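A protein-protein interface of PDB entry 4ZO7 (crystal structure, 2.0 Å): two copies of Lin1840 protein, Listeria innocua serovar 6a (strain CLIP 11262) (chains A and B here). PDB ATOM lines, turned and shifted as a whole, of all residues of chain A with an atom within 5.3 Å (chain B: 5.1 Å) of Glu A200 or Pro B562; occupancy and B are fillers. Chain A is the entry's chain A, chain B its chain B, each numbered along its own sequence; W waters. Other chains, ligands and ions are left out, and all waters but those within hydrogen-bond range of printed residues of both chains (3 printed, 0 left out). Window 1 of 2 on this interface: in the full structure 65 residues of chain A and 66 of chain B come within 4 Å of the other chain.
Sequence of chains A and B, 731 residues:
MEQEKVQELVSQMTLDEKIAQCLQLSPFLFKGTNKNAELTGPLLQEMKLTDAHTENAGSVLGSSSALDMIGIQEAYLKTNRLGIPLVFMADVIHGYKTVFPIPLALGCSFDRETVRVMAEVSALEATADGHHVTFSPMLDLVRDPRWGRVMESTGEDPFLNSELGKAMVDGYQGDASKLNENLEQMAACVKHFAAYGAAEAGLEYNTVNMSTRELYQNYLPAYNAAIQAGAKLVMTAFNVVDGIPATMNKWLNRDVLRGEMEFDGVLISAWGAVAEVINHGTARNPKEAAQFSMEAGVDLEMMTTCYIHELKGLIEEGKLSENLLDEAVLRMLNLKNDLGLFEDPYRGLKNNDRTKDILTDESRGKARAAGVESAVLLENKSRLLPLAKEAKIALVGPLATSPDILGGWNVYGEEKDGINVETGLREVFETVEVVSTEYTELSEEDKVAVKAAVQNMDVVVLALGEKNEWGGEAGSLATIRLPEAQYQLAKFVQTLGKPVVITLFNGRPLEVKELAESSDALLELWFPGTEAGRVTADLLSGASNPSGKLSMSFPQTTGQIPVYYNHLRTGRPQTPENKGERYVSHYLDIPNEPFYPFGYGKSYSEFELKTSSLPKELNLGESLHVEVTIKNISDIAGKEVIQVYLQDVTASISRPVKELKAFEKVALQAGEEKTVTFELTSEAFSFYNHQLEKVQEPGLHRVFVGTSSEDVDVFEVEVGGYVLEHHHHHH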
ATOM      1  N   ASP A 144     -35.538 -13.822 -27.625  1.00  0.00           N
ATOM      2  CA  ASP A 144     -34.590 -14.155 -28.690  1.00  0.00           C
ATOM      3  C   ASP A 144     -34.561 -15.668 -28.915  1.00  0.00           C
ATOM      4  O   ASP A 144     -33.863 -16.412 -28.251  1.00  0.00           O
ATOM      5  CB  ASP A 144     -33.196 -13.582 -28.383  1.00  0.00           C
ATOM      6  CG  ASP A 144     -32.254 -13.715 -29.552  1.00  0.00           C
ATOM      7  OD1 ASP A 144     -32.574 -14.518 -30.510  1.00  0.00           O
ATOM      8  OD2 ASP A 144     -31.215 -12.998 -29.514  1.00  0.00           O
ATOM      9  N   ALA A 198     -31.211 -12.591 -22.126  1.00  0.00           N
ATOM     10  CA  ALA A 198     -30.937 -11.474 -23.004  1.00  0.00           C
ATOM     11  C   ALA A 198     -29.576 -11.634 -23.767  1.00  0.00           C
ATOM     12  O   ALA A 198     -29.100 -10.652 -24.400  1.00  0.00           O
ATOM     13  CB  ALA A 198     -30.979 -10.185 -22.188  1.00  0.00           C
ATOM     14  N   ALA A 199     -28.978 -12.843 -23.760  1.00  0.00           N
ATOM     15  CA  ALA A 199     -27.671 -13.100 -24.418  1.00  0.00           C
ATOM     16  C   ALA A 199     -27.634 -12.484 -25.809  1.00  0.00           C
ATOM     17  O   ALA A 199     -28.505 -12.771 -26.653  1.00  0.00           O
ATOM     18  CB  ALA A 199     -27.347 -14.584 -24.545  1.00  0.00           C
ATOM     19  N   GLU A 200     -26.598 -11.682 -26.030  1.00  0.00           N
ATOM     20  CA  GLU A 200     -26.469 -10.951 -27.241  1.00  0.00           C
ATOM     21  C   GLU A 200     -26.386 -11.930 -28.440  1.00  0.00           C
ATOM     22  O   GLU A 200     -25.682 -12.941 -28.354  1.00  0.00           O
ATOM     23  CB  GLU A 200     -25.208 -10.060 -27.201  1.00  0.00           C
ATOM     24  CG  GLU A 200     -25.277  -8.894 -28.170  1.00  0.00           C
ATOM     25  CD  GLU A 200     -24.349  -7.751 -27.765  1.00  0.00           C
ATOM     26  OE1 GLU A 200     -23.190  -7.901 -28.135  1.00  0.00           O
ATOM     27  OE2 GLU A 200     -24.761  -6.764 -27.070  1.00  0.00           O
ATOM     28  N   ALA A 201     -27.091 -11.590 -29.510  1.00  0.00           N
ATOM     29  CA  ALA A 201     -27.174 -12.376 -30.788  1.00  0.00           C
ATOM     30  C   ALA A 201     -27.604 -13.833 -30.599  1.00  0.00           C
ATOM     31  O   ALA A 201     -27.341 -14.683 -31.485  1.00  0.00           O
ATOM     32  CB  ALA A 201     -25.870 -12.299 -31.588  1.00  0.00           C
ATOM     33  N   GLY A 202     -28.286 -14.090 -29.487  1.00  0.00           N
ATOM     34  CA  GLY A 202     -28.702 -15.459 -29.090  1.00  0.00           C
ATOM     35  C   GLY A 202     -27.567 -16.452 -28.822  1.00  0.00           C
ATOM     36  O   GLY A 202     -27.778 -17.625 -28.786  1.00  0.00           O
ATOM     37  N   LEU A 203     -26.343 -15.969 -28.688  1.00  0.00           N
ATOM     38  CA  LEU A 203     -25.177 -16.851 -28.555  1.00  0.00           C
ATOM     39  C   LEU A 203     -24.986 -17.316 -27.115  1.00  0.00           C
ATOM     40  O   LEU A 203     -24.989 -16.532 -26.169  1.00  0.00           O
ATOM     41  CB  LEU A 203     -23.960 -16.126 -29.080  1.00  0.00           C
ATOM     42  CG  LEU A 203     -22.581 -16.753 -29.025  1.00  0.00           C
ATOM     43  CD1 LEU A 203     -22.502 -17.987 -29.909  1.00  0.00           C
ATOM     44  CD2 LEU A 203     -21.595 -15.677 -29.503  1.00  0.00           C
ATOM     45  N   ASN A 206     -23.226 -15.415 -23.997  1.00  0.00           N
ATOM     46  CA  ASN A 206     -22.716 -14.150 -24.454  1.00  0.00           C
ATOM     47  C   ASN A 206     -23.168 -13.007 -23.529  1.00  0.00           C
ATOM     48  O   ASN A 206     -24.123 -13.142 -22.719  1.00  0.00           O
ATOM     49  CB  ASN A 206     -23.132 -13.903 -25.927  1.00  0.00           C
ATOM     50  CG  ASN A 206     -22.202 -12.959 -26.683  1.00  0.00           C
ATOM     51  OD1 ASN A 206     -21.056 -12.690 -26.285  1.00  0.00           O
ATOM     52  ND2 ASN A 206     -22.703 -12.436 -27.782  1.00  0.00           N
ATOM     53  N   THR A 207     -22.473 -11.886 -23.709  1.00  0.00           N
ATOM     54  CA  THR A 207     -22.770 -10.581 -23.124  1.00  0.00           C
ATOM     55  C   THR A 207     -24.261 -10.267 -23.020  1.00  0.00           C
ATOM     56  O   THR A 207     -25.027 -10.440 -23.958  1.00  0.00           O
ATOM     57  CB  THR A 207     -22.190  -9.544 -24.039  1.00  0.00           C
ATOM     58  OG1 THR A 207     -20.771  -9.780 -24.126  1.00  0.00           O
ATOM     59  CG2 THR A 207     -22.513  -8.105 -23.539  1.00  0.00           C
ATOM     60  N   VAL A 208     -24.659  -9.825 -21.834  1.00  0.00           N
ATOM     61  CA  VAL A 208     -25.954  -9.208 -21.629  1.00  0.00           C
ATOM     62  C   VAL A 208     -25.729  -7.753 -21.237  1.00  0.00           C
ATOM     63  O   VAL A 208     -24.850  -7.471 -20.400  1.00  0.00           O
ATOM     64  CB  VAL A 208     -26.691  -9.917 -20.468  1.00  0.00           C
ATOM     65  CG1 VAL A 208     -27.880  -9.089 -20.013  1.00  0.00           C
ATOM     66  CG2 VAL A 208     -27.150 -11.319 -20.892  1.00  0.00           C
ATOM     67  N   ARG B 143     -23.543  -1.190 -34.871  1.00  0.00           N
ATOM     68  CA  ARG B 143     -23.270  -2.666 -34.786  1.00  0.00           C
ATOM     69  C   ARG B 143     -24.286  -3.540 -35.516  1.00  0.00           C
ATOM     70  O   ARG B 143     -24.254  -4.769 -35.369  1.00  0.00           O
ATOM     71  CB  ARG B 143     -23.269  -3.078 -33.360  1.00  0.00           C
ATOM     72  CG  ARG B 143     -22.205  -2.406 -32.522  1.00  0.00           C
ATOM     73  CD  ARG B 143     -22.317  -2.856 -31.088  1.00  0.00           C
ATOM     74  NE  ARG B 143     -21.130  -2.436 -30.382  1.00  0.00           N
ATOM     75  CZ  ARG B 143     -21.007  -2.440 -29.065  1.00  0.00           C
ATOM     76  NH1 ARG B 143     -22.005  -2.871 -28.295  1.00  0.00           N
ATOM     77  NH2 ARG B 143     -19.866  -2.074 -28.506  1.00  0.00           N
ATOM     78  N   GLN B 560     -26.346 -13.594 -37.077  1.00  0.00           N
ATOM     79  CA  GLN B 560     -25.116 -13.392 -36.283  1.00  0.00           C
ATOM     80  C   GLN B 560     -25.077 -12.006 -35.627  1.00  0.00           C
ATOM     81  O   GLN B 560     -24.308 -11.764 -34.737  1.00  0.00           O
ATOM     82  CB  GLN B 560     -23.891 -13.569 -37.152  1.00  0.00           C
ATOM     83  CG  GLN B 560     -22.601 -13.737 -36.387  1.00  0.00           C
ATOM     84  CD  GLN B 560     -21.403 -13.940 -37.307  1.00  0.00           C
ATOM     85  OE1 GLN B 560     -21.210 -13.222 -38.295  1.00  0.00           O
ATOM     86  NE2 GLN B 560     -20.611 -14.908 -36.984  1.00  0.00           N
ATOM     87  N   ILE B 561     -25.969 -11.130 -36.051  1.00  0.00           N
ATOM     88  CA  ILE B 561     -25.946  -9.711 -35.696  1.00  0.00           C
ATOM     89  C   ILE B 561     -26.437  -9.527 -34.229  1.00  0.00           C
ATOM     90  O   ILE B 561     -27.424 -10.118 -33.824  1.00  0.00           O
ATOM     91  CB  ILE B 561     -26.925  -8.930 -36.644  1.00  0.00           C
ATOM     92  CG1 ILE B 561     -26.314  -8.838 -38.019  1.00  0.00           C
ATOM     93  CG2 ILE B 561     -27.219  -7.523 -36.161  1.00  0.00           C
ATOM     94  CD1 ILE B 561     -27.257  -8.364 -39.117  1.00  0.00           C
ATOM     95  N   PRO B 562     -25.777  -8.659 -33.475  1.00  0.00           N
ATOM     96  CA  PRO B 562     -24.605  -7.833 -33.774  1.00  0.00           C
ATOM     97  C   PRO B 562     -23.338  -8.620 -33.597  1.00  0.00           C
ATOM     98  O   PRO B 562     -23.209  -9.389 -32.677  1.00  0.00           O
ATOM     99  CB  PRO B 562     -24.720  -6.718 -32.756  1.00  0.00           C
ATOM    100  CG  PRO B 562     -25.274  -7.440 -31.571  1.00  0.00           C
ATOM    101  CD  PRO B 562     -26.351  -8.283 -32.182  1.00  0.00           C
ATOM    102  N   VAL B 563     -22.410  -8.459 -34.518  1.00  0.00           N
ATOM    103  CA  VAL B 563     -21.090  -9.096 -34.405  1.00  0.00           C
ATOM    104  C   VAL B 563     -20.121  -7.965 -34.620  1.00  0.00           C
ATOM    105  O   VAL B 563     -20.368  -7.139 -35.451  1.00  0.00           O
ATOM    106  CB  VAL B 563     -20.931 -10.264 -35.438  1.00  0.00           C
ATOM    107  CG1 VAL B 563     -21.216  -9.816 -36.852  1.00  0.00           C
ATOM    108  CG2 VAL B 563     -19.579 -10.917 -35.359  1.00  0.00           C
ATOM    109  N   TYR B 564     -19.060  -7.897 -33.839  1.00  0.00           N
ATOM    110  CA  TYR B 564     -18.194  -6.706 -33.846  1.00  0.00           C
ATOM    111  C   TYR B 564     -16.900  -7.051 -33.147  1.00  0.00           C
ATOM    112  O   TYR B 564     -16.913  -7.891 -32.239  1.00  0.00           O
ATOM    113  CB  TYR B 564     -18.854  -5.491 -33.183  1.00  0.00           C
ATOM    114  CG  TYR B 564     -19.487  -5.772 -31.827  1.00  0.00           C
ATOM    115  CD1 TYR B 564     -20.810  -6.237 -31.700  1.00  0.00           C
ATOM    116  CD2 TYR B 564     -18.733  -5.640 -30.660  1.00  0.00           C
ATOM    117  CE1 TYR B 564     -21.346  -6.517 -30.418  1.00  0.00           C
ATOM    118  CE2 TYR B 564     -19.273  -5.902 -29.395  1.00  0.00           C
ATOM    119  CZ  TYR B 564     -20.568  -6.343 -29.287  1.00  0.00           C
ATOM    120  OH  TYR B 564     -21.038  -6.602 -28.027  1.00  0.00           O
ATOM    121  N   TYR B 587     -22.180 -21.028 -32.004  1.00  0.00           N
ATOM    122  CA  TYR B 587     -23.359 -21.417 -32.690  1.00  0.00           C
ATOM    123  C   TYR B 587     -23.246 -22.852 -33.237  1.00  0.00           C
ATOM    124  O   TYR B 587     -22.188 -23.243 -33.718  1.00  0.00           O
ATOM    125  CB  TYR B 587     -23.598 -20.500 -33.897  1.00  0.00           C
ATOM    126  CG  TYR B 587     -23.986 -19.061 -33.564  1.00  0.00           C
ATOM    127  CD1 TYR B 587     -25.306 -18.729 -33.117  1.00  0.00           C
ATOM    128  CD2 TYR B 587     -23.079 -18.068 -33.697  1.00  0.00           C
ATOM    129  CE1 TYR B 587     -25.655 -17.394 -32.879  1.00  0.00           C
ATOM    130  CE2 TYR B 587     -23.425 -16.739 -33.443  1.00  0.00           C
ATOM    131  CZ  TYR B 587     -24.698 -16.429 -33.032  1.00  0.00           C
ATOM    132  OH  TYR B 587     -24.942 -15.143 -32.701  1.00  0.00           O
HETATM  133  O   HOH W   1     -21.918 -11.715 -31.027  1.00  0.00           O
HETATM  134  O   HOH W   2     -19.685  -8.592 -26.270  1.00  0.00           O
HETATM  135  O   HOH W   3     -24.477  -4.470 -28.933  1.00  0.00           O
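No position is printed for both chains.
Of the 6 pairs that touch across the chains among the printed residues, none has its exchanged pair printed and touching as well.
ND2 of Asn A206 lies within hydrogen-bond range of O of Glu A200, at 3.1 Å.
The backbone carbonyl oxygen (O) of Thr A207 sits at hydrogen-bond distance from the backbone NH (N) of Glu A200, 2.9 Å away.
Glu A200 touches two residues of chain B.
Of the printed residues of chain B, Leu A203 touches Tyr B587 (3.7 Å).
Of the printed residues of chain A, Ile B561 touches Ala A201 (3.5 Å).
Printed residues of chain B within 4 Å of Ala A201: Gln B560, Ile B561 and Tyr B587.
Of the printed residues of chain A, Tyr B564 touches Glu A200 (2.5 Å).
Printed residues of chain A within 4 Å of Gln B560: Ala A201 (3.6 Å).
Gly A202 touches none of the printed residues of chain B.
The nearest printed residue of chain A that does not touch Gln B560 is Glu A200 (6.6 Å).
Of the 7 printed residues of chain B, 5 touch a printed residue of chain A.
Among the printed residues, 6 pairs touch across the chains.
Among the printed residues, no Asp or Glu carboxylate lies within 4 Å of a Lys or Arg side-chain nitrogen of the other chain.
Water W2 lies within hydrogen-bond range of OG1 of Thr A207 (2.7 Å) and OH of Tyr B564 (3.0 Å).
Water W3 lies within hydrogen-bond range of OE2 of Glu A200 and NH1 of Arg B143.
Water W1 bridges O of Pro B562 and ND2 of Asn A206.
The side-chain carboxylate (OE1) of Glu A200 lies within hydrogen-bond range of the side-chain hydroxyl (OH) of Tyr B564, 2.5 Å away.
The side-chain hydroxyl of Tyr B587 is in hydrogen-bond range of the backbone carbonyl oxygen of Ala A201, 2.7 Å away.
CG of Glu A200 touches CG of Pro B562, 3.7 Å away.
O of Gln B560 touches CB of Ala A201, 3.6 Å away.
Ile B561 touches Ala A201 (O to CB, 3.5 Å).
Tyr B587 touches Leu A203 (N to CD1, 3.7 Å).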
